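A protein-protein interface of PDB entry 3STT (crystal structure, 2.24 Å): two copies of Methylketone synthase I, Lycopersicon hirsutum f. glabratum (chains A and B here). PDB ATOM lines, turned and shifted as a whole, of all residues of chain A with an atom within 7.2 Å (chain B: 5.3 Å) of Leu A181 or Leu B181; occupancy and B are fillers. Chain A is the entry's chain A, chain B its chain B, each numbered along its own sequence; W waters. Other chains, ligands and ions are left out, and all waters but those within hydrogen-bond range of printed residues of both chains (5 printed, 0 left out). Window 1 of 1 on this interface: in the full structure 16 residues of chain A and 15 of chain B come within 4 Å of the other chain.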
ATOM      1  N   PHE A  22       6.963  22.715  -3.780  1.00  0.00           N
ATOM      2  CA  PHE A  22       8.364  22.417  -4.050  1.00  0.00           C
ATOM      3  C   PHE A  22       9.045  23.412  -4.969  1.00  0.00           C
ATOM      4  O   PHE A  22      10.271  23.439  -5.043  1.00  0.00           O
ATOM      5  CB  PHE A  22       8.513  21.028  -4.673  1.00  0.00           C
ATOM      6  CG  PHE A  22       7.648  19.986  -4.047  1.00  0.00           C
ATOM      7  CD1 PHE A  22       7.720  19.726  -2.683  1.00  0.00           C
ATOM      8  CD2 PHE A  22       6.754  19.255  -4.830  1.00  0.00           C
ATOM      9  CE1 PHE A  22       6.911  18.746  -2.104  1.00  0.00           C
ATOM     10  CE2 PHE A  22       5.943  18.277  -4.264  1.00  0.00           C
ATOM     11  CZ  PHE A  22       6.021  18.022  -2.895  1.00  0.00           C
ATOM     12  N   HIS A  23       8.268  24.230  -5.670  1.00  0.00           N
ATOM     13  CA  HIS A  23       8.878  25.170  -6.597  1.00  0.00           C
ATOM     14  C   HIS A  23       9.109  26.576  -6.072  1.00  0.00           C
ATOM     15  O   HIS A  23       9.105  26.808  -4.865  1.00  0.00           O
ATOM     16  CB  HIS A  23       8.068  25.206  -7.899  1.00  0.00           C
ATOM     17  CG  HIS A  23       8.148  23.930  -8.677  1.00  0.00           C
ATOM     18  ND1 HIS A  23       7.580  22.752  -8.237  1.00  0.00           N
ATOM     19  CD2 HIS A  23       8.778  23.633  -9.839  1.00  0.00           C
ATOM     20  CE1 HIS A  23       7.857  21.786  -9.096  1.00  0.00           C
ATOM     21  NE2 HIS A  23       8.584  22.294 -10.076  1.00  0.00           N
ATOM     22  N   GLY A  24       9.340  27.506  -6.994  1.00  0.00           N
ATOM     23  CA  GLY A  24       9.575  28.890  -6.630  1.00  0.00           C
ATOM     24  C   GLY A  24       9.464  29.784  -7.851  1.00  0.00           C
ATOM     25  O   GLY A  24       9.133  29.309  -8.936  1.00  0.00           O
ATOM     26  N   ALA A  25       9.753  31.071  -7.677  1.00  0.00           N
ATOM     27  CA  ALA A  25       9.687  32.043  -8.760  1.00  0.00           C
ATOM     28  C   ALA A  25      10.516  31.590  -9.959  1.00  0.00           C
ATOM     29  O   ALA A  25      10.171  31.866 -11.107  1.00  0.00           O
ATOM     30  CB  ALA A  25      10.188  33.412  -8.266  1.00  0.00           C
ATOM     31  N   TRP A  26      11.610  30.893  -9.678  1.00  0.00           N
ATOM     32  CA  TRP A  26      12.504  30.397 -10.715  1.00  0.00           C
ATOM     33  C   TRP A  26      11.853  29.536 -11.811  1.00  0.00           C
ATOM     34  O   TRP A  26      12.302  29.544 -12.952  1.00  0.00           O
ATOM     35  CB  TRP A  26      13.641  29.594 -10.075  1.00  0.00           C
ATOM     36  CG  TRP A  26      13.180  28.407  -9.255  1.00  0.00           C
ATOM     37  CD1 TRP A  26      12.952  28.380  -7.909  1.00  0.00           C
ATOM     38  CD2 TRP A  26      12.875  27.089  -9.733  1.00  0.00           C
ATOM     39  NE1 TRP A  26      12.528  27.132  -7.517  1.00  0.00           N
ATOM     40  CE2 TRP A  26      12.469  26.315  -8.624  1.00  0.00           C
ATOM     41  CE3 TRP A  26      12.903  26.478 -11.000  1.00  0.00           C
ATOM     42  CZ2 TRP A  26      12.094  24.969  -8.729  1.00  0.00           C
ATOM     43  CZ3 TRP A  26      12.528  25.131 -11.105  1.00  0.00           C
ATOM     44  CH2 TRP A  26      12.130  24.399  -9.976  1.00  0.00           C
ATOM     45  N   CYS A  27      10.804  28.791 -11.476  1.00  0.00           N
ATOM     46  CA  CYS A  27      10.185  27.920 -12.467  1.00  0.00           C
ATOM     47  C   CYS A  27       9.508  28.683 -13.601  1.00  0.00           C
ATOM     48  O   CYS A  27       9.248  28.112 -14.661  1.00  0.00           O
ATOM     49  CB  CYS A  27       9.179  26.970 -11.803  1.00  0.00           C
ATOM     50  SG  CYS A  27       7.595  27.715 -11.371  1.00  0.00           S
ATOM     51  N   TYR A  29      10.883  31.222 -15.142  1.00  0.00           N
ATOM     52  CA  TYR A  29      11.893  31.975 -15.885  1.00  0.00           C
ATOM     53  C   TYR A  29      11.652  32.204 -17.378  1.00  0.00           C
ATOM     54  O   TYR A  29      11.935  33.291 -17.884  1.00  0.00           O
ATOM     55  CB  TYR A  29      13.296  31.391 -15.638  1.00  0.00           C
ATOM     56  CG  TYR A  29      13.675  30.156 -16.427  1.00  0.00           C
ATOM     57  CD1 TYR A  29      14.615  30.231 -17.454  1.00  0.00           C
ATOM     58  CD2 TYR A  29      13.138  28.910 -16.118  1.00  0.00           C
ATOM     59  CE1 TYR A  29      15.020  29.091 -18.150  1.00  0.00           C
ATOM     60  CE2 TYR A  29      13.531  27.762 -16.811  1.00  0.00           C
ATOM     61  CZ  TYR A  29      14.475  27.862 -17.823  1.00  0.00           C
ATOM     62  OH  TYR A  29      14.887  26.734 -18.497  1.00  0.00           O
ATOM     63  N   ASP A  46       8.237  34.023  -4.564  1.00  0.00           N
ATOM     64  CA  ASP A  46       8.629  32.796  -3.874  1.00  0.00           C
ATOM     65  C   ASP A  46       7.712  32.776  -2.658  1.00  0.00           C
ATOM     66  O   ASP A  46       7.688  33.745  -1.891  1.00  0.00           O
ATOM     67  CB  ASP A  46      10.067  32.846  -3.337  1.00  0.00           C
ATOM     68  CG  ASP A  46      11.107  32.567  -4.390  1.00  0.00           C
ATOM     69  OD1 ASP A  46      10.834  31.785  -5.319  1.00  0.00           O
ATOM     70  OD2 ASP A  46      12.219  33.117  -4.270  1.00  0.00           O
ATOM     71  N   SER A  50      10.251  28.655  -0.169  1.00  0.00           N
ATOM     72  CA  SER A  50      10.283  28.244  -1.567  1.00  0.00           C
ATOM     73  C   SER A  50      11.346  29.064  -2.300  1.00  0.00           C
ATOM     74  O   SER A  50      11.598  30.214  -1.952  1.00  0.00           O
ATOM     75  CB  SER A  50       8.911  28.476  -2.217  1.00  0.00           C
ATOM     76  OG  SER A  50       7.872  27.870  -1.458  1.00  0.00           O
ATOM     77  N   GLY A  51      11.965  28.476  -3.316  1.00  0.00           N
ATOM     78  CA  GLY A  51      12.985  29.203  -4.044  1.00  0.00           C
ATOM     79  C   GLY A  51      14.032  29.717  -3.074  1.00  0.00           C
ATOM     80  O   GLY A  51      14.601  28.944  -2.302  1.00  0.00           O
ATOM     81  N   ILE A  52      14.287  31.021  -3.099  1.00  0.00           N
ATOM     82  CA  ILE A  52      15.271  31.591  -2.197  1.00  0.00           C
ATOM     83  C   ILE A  52      14.642  32.331  -1.019  1.00  0.00           C
ATOM     84  O   ILE A  52      15.275  33.185  -0.395  1.00  0.00           O
ATOM     85  CB  ILE A  52      16.252  32.536  -2.938  1.00  0.00           C
ATOM     86  CG1 ILE A  52      15.482  33.630  -3.678  1.00  0.00           C
ATOM     87  CG2 ILE A  52      17.112  31.721  -3.905  1.00  0.00           C
ATOM     88  CD1 ILE A  52      16.353  34.782  -4.133  1.00  0.00           C
ATOM     89  N   LEU A 175      14.528  19.558 -15.995  1.00  0.00           N
ATOM     90  CA  LEU A 175      14.390  18.537 -14.981  1.00  0.00           C
ATOM     91  C   LEU A 175      15.582  18.698 -14.051  1.00  0.00           C
ATOM     92  O   LEU A 175      15.436  18.707 -12.827  1.00  0.00           O
ATOM     93  CB  LEU A 175      14.397  17.134 -15.591  1.00  0.00           C
ATOM     94  CG  LEU A 175      14.580  15.969 -14.606  1.00  0.00           C
ATOM     95  CD1 LEU A 175      13.522  16.011 -13.500  1.00  0.00           C
ATOM     96  CD2 LEU A 175      14.515  14.660 -15.375  1.00  0.00           C
ATOM     97  N   ALA A 176      16.772  18.834 -14.635  1.00  0.00           N
ATOM     98  CA  ALA A 176      18.011  19.007 -13.853  1.00  0.00           C
ATOM     99  C   ALA A 176      17.918  20.266 -12.999  1.00  0.00           C
ATOM    100  O   ALA A 176      18.284  20.248 -11.829  1.00  0.00           O
ATOM    101  CB  ALA A 176      19.216  19.085 -14.804  1.00  0.00           C
ATOM    102  N   LEU A 177      17.434  21.352 -13.599  1.00  0.00           N
ATOM    103  CA  LEU A 177      17.278  22.622 -12.901  1.00  0.00           C
ATOM    104  C   LEU A 177      16.413  22.427 -11.658  1.00  0.00           C
ATOM    105  O   LEU A 177      16.769  22.859 -10.557  1.00  0.00           O
ATOM    106  CB  LEU A 177      16.620  23.650 -13.834  1.00  0.00           C
ATOM    107  CG  LEU A 177      16.319  25.039 -13.250  1.00  0.00           C
ATOM    108  CD1 LEU A 177      17.614  25.686 -12.771  1.00  0.00           C
ATOM    109  CD2 LEU A 177      15.643  25.915 -14.306  1.00  0.00           C
ATOM    110  N   ALA A 178      15.273  21.769 -11.852  1.00  0.00           N
ATOM    111  CA  ALA A 178      14.326  21.497 -10.777  1.00  0.00           C
ATOM    112  C   ALA A 178      14.915  20.650  -9.657  1.00  0.00           C
ATOM    113  O   ALA A 178      14.690  20.929  -8.473  1.00  0.00           O
ATOM    114  CB  ALA A 178      13.083  20.807 -11.343  1.00  0.00           C
ATOM    115  N   THR A 179      15.666  19.613 -10.022  1.00  0.00           N
ATOM    116  CA  THR A 179      16.264  18.742  -9.018  1.00  0.00           C
ATOM    117  C   THR A 179      17.265  19.490  -8.152  1.00  0.00           C
ATOM    118  O   THR A 179      17.531  19.093  -7.020  1.00  0.00           O
ATOM    119  CB  THR A 179      16.966  17.521  -9.662  1.00  0.00           C
ATOM    120  OG1 THR A 179      18.021  17.966 -10.526  1.00  0.00           O
ATOM    121  CG2 THR A 179      15.970  16.710 -10.466  1.00  0.00           C
ATOM    122  N   ALA A 180      17.822  20.574  -8.680  1.00  0.00           N
ATOM    123  CA  ALA A 180      18.789  21.365  -7.924  1.00  0.00           C
ATOM    124  C   ALA A 180      18.096  22.478  -7.140  1.00  0.00           C
ATOM    125  O   ALA A 180      18.730  23.167  -6.343  1.00  0.00           O
ATOM    126  CB  ALA A 180      19.816  21.973  -8.871  1.00  0.00           C
ATOM    127  N   LEU A 181      16.795  22.648  -7.355  1.00  0.00           N
ATOM    128  CA  LEU A 181      16.065  23.729  -6.695  1.00  0.00           C
ATOM    129  C   LEU A 181      14.816  23.389  -5.881  1.00  0.00           C
ATOM    130  O   LEU A 181      14.409  24.197  -5.035  1.00  0.00           O
ATOM    131  CB  LEU A 181      15.698  24.788  -7.734  1.00  0.00           C
ATOM    132  CG  LEU A 181      16.860  25.504  -8.428  1.00  0.00           C
ATOM    133  CD1 LEU A 181      16.319  26.313  -9.612  1.00  0.00           C
ATOM    134  CD2 LEU A 181      17.578  26.413  -7.432  1.00  0.00           C
ATOM    135  N   VAL A 182      14.194  22.231  -6.134  1.00  0.00           N
ATOM    136  CA  VAL A 182      12.999  21.865  -5.372  1.00  0.00           C
ATOM    137  C   VAL A 182      13.283  21.823  -3.887  1.00  0.00           C
ATOM    138  O   VAL A 182      14.333  21.337  -3.469  1.00  0.00           O
ATOM    139  CB  VAL A 182      12.379  20.498  -5.808  1.00  0.00           C
ATOM    140  CG1 VAL A 182      11.768  20.660  -7.213  1.00  0.00           C
ATOM    141  CG2 VAL A 182      13.409  19.339  -5.688  1.00  0.00           C
ATOM    142  N   ARG A 183      12.355  22.352  -3.094  1.00  0.00           N
ATOM    143  CA  ARG A 183      12.513  22.365  -1.641  1.00  0.00           C
ATOM    144  C   ARG A 183      11.315  21.697  -0.979  1.00  0.00           C
ATOM    145  O   ARG A 183      10.248  21.569  -1.580  1.00  0.00           O
ATOM    146  CB  ARG A 183      12.655  23.796  -1.118  1.00  0.00           C
ATOM    147  CG  ARG A 183      13.884  24.539  -1.647  1.00  0.00           C
ATOM    148  CD  ARG A 183      13.910  25.971  -1.136  1.00  0.00           C
ATOM    149  NE  ARG A 183      13.993  26.021   0.323  1.00  0.00           N
ATOM    150  CZ  ARG A 183      13.904  27.135   1.047  1.00  0.00           C
ATOM    151  NH1 ARG A 183      13.725  28.315   0.454  1.00  0.00           N
ATOM    152  NH2 ARG A 183      13.997  27.070   2.369  1.00  0.00           N
ATOM    153  N   PRO A 184      11.475  21.271   0.279  1.00  0.00           N
ATOM    154  CA  PRO A 184      10.393  20.610   1.009  1.00  0.00           C
ATOM    155  C   PRO A 184       9.147  21.472   1.188  1.00  0.00           C
ATOM    156  O   PRO A 184       9.226  22.698   1.276  1.00  0.00           O
ATOM    157  CB  PRO A 184      11.035  20.269   2.356  1.00  0.00           C
ATOM    158  CG  PRO A 184      12.518  20.194   2.037  1.00  0.00           C
ATOM    159  CD  PRO A 184      12.700  21.344   1.093  1.00  0.00           C
ATOM    160  N   PHE B  22      27.172  34.592  -5.506  1.00  0.00           N
ATOM    161  CA  PHE B  22      25.739  34.819  -5.715  1.00  0.00           C
ATOM    162  C   PHE B  22      24.986  33.659  -6.347  1.00  0.00           C
ATOM    163  O   PHE B  22      23.755  33.599  -6.275  1.00  0.00           O
ATOM    164  CB  PHE B  22      25.491  36.045  -6.606  1.00  0.00           C
ATOM    165  CG  PHE B  22      26.438  37.186  -6.378  1.00  0.00           C
ATOM    166  CD1 PHE B  22      26.519  37.816  -5.144  1.00  0.00           C
ATOM    167  CD2 PHE B  22      27.225  37.659  -7.421  1.00  0.00           C
ATOM    168  CE1 PHE B  22      27.364  38.907  -4.957  1.00  0.00           C
ATOM    169  CE2 PHE B  22      28.074  38.744  -7.243  1.00  0.00           C
ATOM    170  CZ  PHE B  22      28.144  39.368  -6.010  1.00  0.00           C
ATOM    171  N   TRP B  26      22.275  25.418  -9.268  1.00  0.00           N
ATOM    172  CA  TRP B  26      21.320  25.664 -10.343  1.00  0.00           C
ATOM    173  C   TRP B  26      21.895  26.245 -11.632  1.00  0.00           C
ATOM    174  O   TRP B  26      21.387  25.962 -12.718  1.00  0.00           O
ATOM    175  CB  TRP B  26      20.203  26.591  -9.854  1.00  0.00           C
ATOM    176  CG  TRP B  26      20.682  27.936  -9.362  1.00  0.00           C
ATOM    177  CD1 TRP B  26      20.963  28.284  -8.070  1.00  0.00           C
ATOM    178  CD2 TRP B  26      20.961  29.099 -10.157  1.00  0.00           C
ATOM    179  NE1 TRP B  26      21.390  29.590  -8.011  1.00  0.00           N
ATOM    180  CE2 TRP B  26      21.393  30.115  -9.277  1.00  0.00           C
ATOM    181  CE3 TRP B  26      20.868  29.384 -11.527  1.00  0.00           C
ATOM    182  CZ2 TRP B  26      21.758  31.391  -9.724  1.00  0.00           C
ATOM    183  CZ3 TRP B  26      21.229  30.656 -11.973  1.00  0.00           C
ATOM    184  CH2 TRP B  26      21.661  31.645 -11.071  1.00  0.00           C
ATOM    185  N   GLY B  51      22.278  29.086  -3.583  1.00  0.00           N
ATOM    186  CA  GLY B  51      21.208  28.223  -4.065  1.00  0.00           C
ATOM    187  C   GLY B  51      20.173  27.961  -2.990  1.00  0.00           C
ATOM    188  O   GLY B  51      19.623  28.908  -2.420  1.00  0.00           O
ATOM    189  N   ILE B  52      19.904  26.688  -2.698  1.00  0.00           N
ATOM    190  CA  ILE B  52      18.932  26.363  -1.662  1.00  0.00           C
ATOM    191  C   ILE B  52      19.595  25.880  -0.375  1.00  0.00           C
ATOM    192  O   ILE B  52      19.002  25.132   0.402  1.00  0.00           O
ATOM    193  CB  ILE B  52      17.908  25.308  -2.132  1.00  0.00           C
ATOM    194  CG1 ILE B  52      18.612  24.007  -2.514  1.00  0.00           C
ATOM    195  CG2 ILE B  52      17.120  25.849  -3.306  1.00  0.00           C
ATOM    196  CD1 ILE B  52      17.638  22.881  -2.838  1.00  0.00           C
ATOM    197  N   LEU B 177      16.245  33.814 -15.040  1.00  0.00           N
ATOM    198  CA  LEU B 177      16.435  32.754 -14.046  1.00  0.00           C
ATOM    199  C   LEU B 177      17.372  33.247 -12.941  1.00  0.00           C
ATOM    200  O   LEU B 177      17.079  33.110 -11.751  1.00  0.00           O
ATOM    201  CB  LEU B 177      17.027  31.501 -14.704  1.00  0.00           C
ATOM    202  CG  LEU B 177      17.299  30.279 -13.807  1.00  0.00           C
ATOM    203  CD1 LEU B 177      16.010  29.773 -13.192  1.00  0.00           C
ATOM    204  CD2 LEU B 177      17.933  29.173 -14.634  1.00  0.00           C
ATOM    205  N   ALA B 178      18.490  33.834 -13.351  1.00  0.00           N
ATOM    206  CA  ALA B 178      19.484  34.360 -12.422  1.00  0.00           C
ATOM    207  C   ALA B 178      18.932  35.424 -11.473  1.00  0.00           C
ATOM    208  O   ALA B 178      19.202  35.390 -10.270  1.00  0.00           O
ATOM    209  CB  ALA B 178      20.670  34.930 -13.202  1.00  0.00           C
ATOM    210  N   THR B 179      18.155  36.365 -12.001  1.00  0.00           N
ATOM    211  CA  THR B 179      17.609  37.430 -11.166  1.00  0.00           C
ATOM    212  C   THR B 179      16.630  36.911 -10.122  1.00  0.00           C
ATOM    213  O   THR B 179      16.386  37.565  -9.107  1.00  0.00           O
ATOM    214  CB  THR B 179      16.913  38.528 -12.019  1.00  0.00           C
ATOM    215  OG1 THR B 179      15.731  37.999 -12.623  1.00  0.00           O
ATOM    216  CG2 THR B 179      17.842  39.010 -13.109  1.00  0.00           C
ATOM    217  N   ALA B 180      16.062  35.737 -10.364  1.00  0.00           N
ATOM    218  CA  ALA B 180      15.131  35.161  -9.407  1.00  0.00           C
ATOM    219  C   ALA B 180      15.847  34.223  -8.439  1.00  0.00           C
ATOM    220  O   ALA B 180      15.227  33.711  -7.509  1.00  0.00           O
ATOM    221  CB  ALA B 180      14.014  34.394 -10.143  1.00  0.00           C
ATOM    222  N   LEU B 181      17.147  34.007  -8.642  1.00  0.00           N
ATOM    223  CA  LEU B 181      17.892  33.078  -7.784  1.00  0.00           C
ATOM    224  C   LEU B 181      19.179  33.571  -7.107  1.00  0.00           C
ATOM    225  O   LEU B 181      19.604  32.990  -6.109  1.00  0.00           O
ATOM    226  CB  LEU B 181      18.234  31.806  -8.573  1.00  0.00           C
ATOM    227  CG  LEU B 181      17.104  30.917  -9.098  1.00  0.00           C
ATOM    228  CD1 LEU B 181      17.627  29.932 -10.161  1.00  0.00           C
ATOM    229  CD2 LEU B 181      16.440  30.222  -7.879  1.00  0.00           C
ATOM    230  N   VAL B 182      19.826  34.601  -7.645  1.00  0.00           N
ATOM    231  CA  VAL B 182      21.062  35.073  -7.027  1.00  0.00           C
ATOM    232  C   VAL B 182      20.816  35.506  -5.593  1.00  0.00           C
ATOM    233  O   VAL B 182      19.786  36.103  -5.281  1.00  0.00           O
ATOM    234  CB  VAL B 182      21.705  36.252  -7.800  1.00  0.00           C
ATOM    235  CG1 VAL B 182      22.179  35.768  -9.169  1.00  0.00           C
ATOM    236  CG2 VAL B 182      20.717  37.412  -7.925  1.00  0.00           C
ATOM    237  N   ARG B 183      21.768  35.195  -4.723  1.00  0.00           N
ATOM    238  CA  ARG B 183      21.656  35.546  -3.313  1.00  0.00           C
ATOM    239  C   ARG B 183      22.873  36.365  -2.905  1.00  0.00           C
ATOM    240  O   ARG B 183      23.875  36.388  -3.615  1.00  0.00           O
ATOM    241  CB  ARG B 183      21.561  34.277  -2.463  1.00  0.00           C
ATOM    242  CG  ARG B 183      20.380  33.378  -2.831  1.00  0.00           C
ATOM    243  CD  ARG B 183      20.377  32.115  -1.990  1.00  0.00           C
ATOM    244  NE  ARG B 183      20.367  32.421  -0.563  1.00  0.00           N
ATOM    245  CZ  ARG B 183      20.510  31.514   0.397  1.00  0.00           C
ATOM    246  NH1 ARG B 183      20.679  30.234   0.087  1.00  0.00           N
ATOM    247  NH2 ARG B 183      20.473  31.887   1.671  1.00  0.00           N
HETATM  248  O   HOH W   1      13.219  31.595  -7.037  1.00  0.00           O
HETATM  249  O   HOH W   2      17.623  33.513   1.604  1.00  0.00           O
HETATM  250  O   HOH W   3      20.838  25.260  -6.317  1.00  0.00           O
HETATM  251  O   HOH W   4      13.058  34.964  -6.151  1.00  0.00           O
HETATM  252  O   HOH W   5      17.286  29.188  -0.983  1.00  0.00           O
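O of Phe A22 is in hydrogen-bond range of N of Arg A183, at 3.1 Å.
The backbone NH of Ile A52 is in hydrogen-bond range of the side-chain carboxylate of Asp A46.
The backbone carbonyl oxygen (O) of Gly A51 sits at hydrogen-bond distance from the guanidinium group (NH1) of Arg A183, 3.0 Å away.
The backbone carbonyl oxygen of Phe B22 lies within hydrogen-bond range of the backbone NH of Arg B183 (3.0 Å).
The backbone carbonyl oxygen (O) of Gly B51 lies within hydrogen-bond range of the guanidinium group (NH1) of Arg B183.
Ala B180 touches Ile A52 (O to CD1, 3.7 Å).
Leu B181 touches Ile A52 (O to CG2, 3.6 Å).
Ile A52 touches Arg B183.
O of Trp B26 touches CD1 of Leu A177, at 3.8 Å.
Leu B177 touches Leu A177.
Ala A180 touches Ile B52 (O to CD1, 3.7 Å).
Trp B26 touches Leu A181 (CB to CD2, 3.6 Å).
CD1 of Leu B181 touches CD1 of Leu A181, 3.9 Å away.
Val A182 touches Ile B52 (O to CD1, 3.7 Å).
CG of Arg A183 touches CG2 of Ile B52, at 3.9 Å.
Leu A175 touches none of the printed residues of chain B.
Of the printed residues of chain B, Leu A177 touches Trp B26 (3.8 Å) and Leu B177 (3.97 Å).
Leu A181 touches three residues of chain B.
Of the printed residues of chain B, Val A182 touches Ile B52.
Of the printed residues of chain A, Leu B177 touches Trp A26, Tyr A29 and Leu A177.
The nearest residue of chain B that does not touch Leu A181 is Leu B177 (5.0 Å).
The nearest residue of chain A that does not touch Leu B181 is Leu A177 (5.0 Å).
The nearest printed residue of chain B that does not touch Ile A52 is Gly B51 (4.1 Å).
Of the 11 printed residues of chain B, 7 touch a printed residue of chain A.
Printed residues of chain B that touch a printed residue of chain A: Trp B26, Ile B52, Leu B177, Ala B180, Leu B181, Val B182 and Arg B183.
Hydrophobic or aromatic side chains of chain B that line the printed part of chain A: Trp B26, Ile B52, Leu B177 and Leu B181.
Of the 21 printed residues of chain A, 8 touch a printed residue of chain B.
Printed residues of chain A that touch a printed residue of chain B: Trp A26, Tyr A29, Ile A52, Leu A177, Ala A180, Leu A181, Val A182 and Arg A183.
Hydrophobic or aromatic side chains of chain A that line the printed part of chain B: Trp A26, Tyr A29, Ile A52, Leu A177 and Leu A181.
Along chain A the printed residues that touch a printed residue of chain B span positions 26 to 183.
Among the printed residues, no Asp or Glu carboxylate lies within 4 Å of a Lys or Arg side-chain nitrogen of the other chain.
Trp A26 touches Leu B177, and with the chains exchanged Leu A177 touches Trp B26.
Ile A52 touches Arg B183, and with the chains exchanged Arg A183 touches Ile B52.
Leu B177 touches its own counterpart, Leu A177.
Leu A181 touches its own counterpart, Leu B181.
Positions printed for both chains: 22, 26, 51, 52, 177, 178, 179, 180, 181, 182 and 183.
Water W5 lies within hydrogen-bond range of O of Gly B51 and O of Gly A51.
Water W4 lies within hydrogen-bond range of the side-chain carboxylate of Asp A46 and the backbone carbonyl oxygen of Ala B180.
Water W1 lies within hydrogen-bond range of the side-chain carboxylate of Asp A46 (2.9 Å), the backbone carbonyl oxygen of Ala B180 (3.0 Å) and the backbone NH of Trp A26 (3.2 Å).
Water W3 lies within hydrogen-bond range of the backbone carbonyl oxygen of Ala A180 (3.0 Å) and the backbone NH of Trp B26 (3.3 Å).
Water W2 lies within hydrogen-bond range of the backbone carbonyl oxygen of Ile A52 and the guanidinium group of Arg B183.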
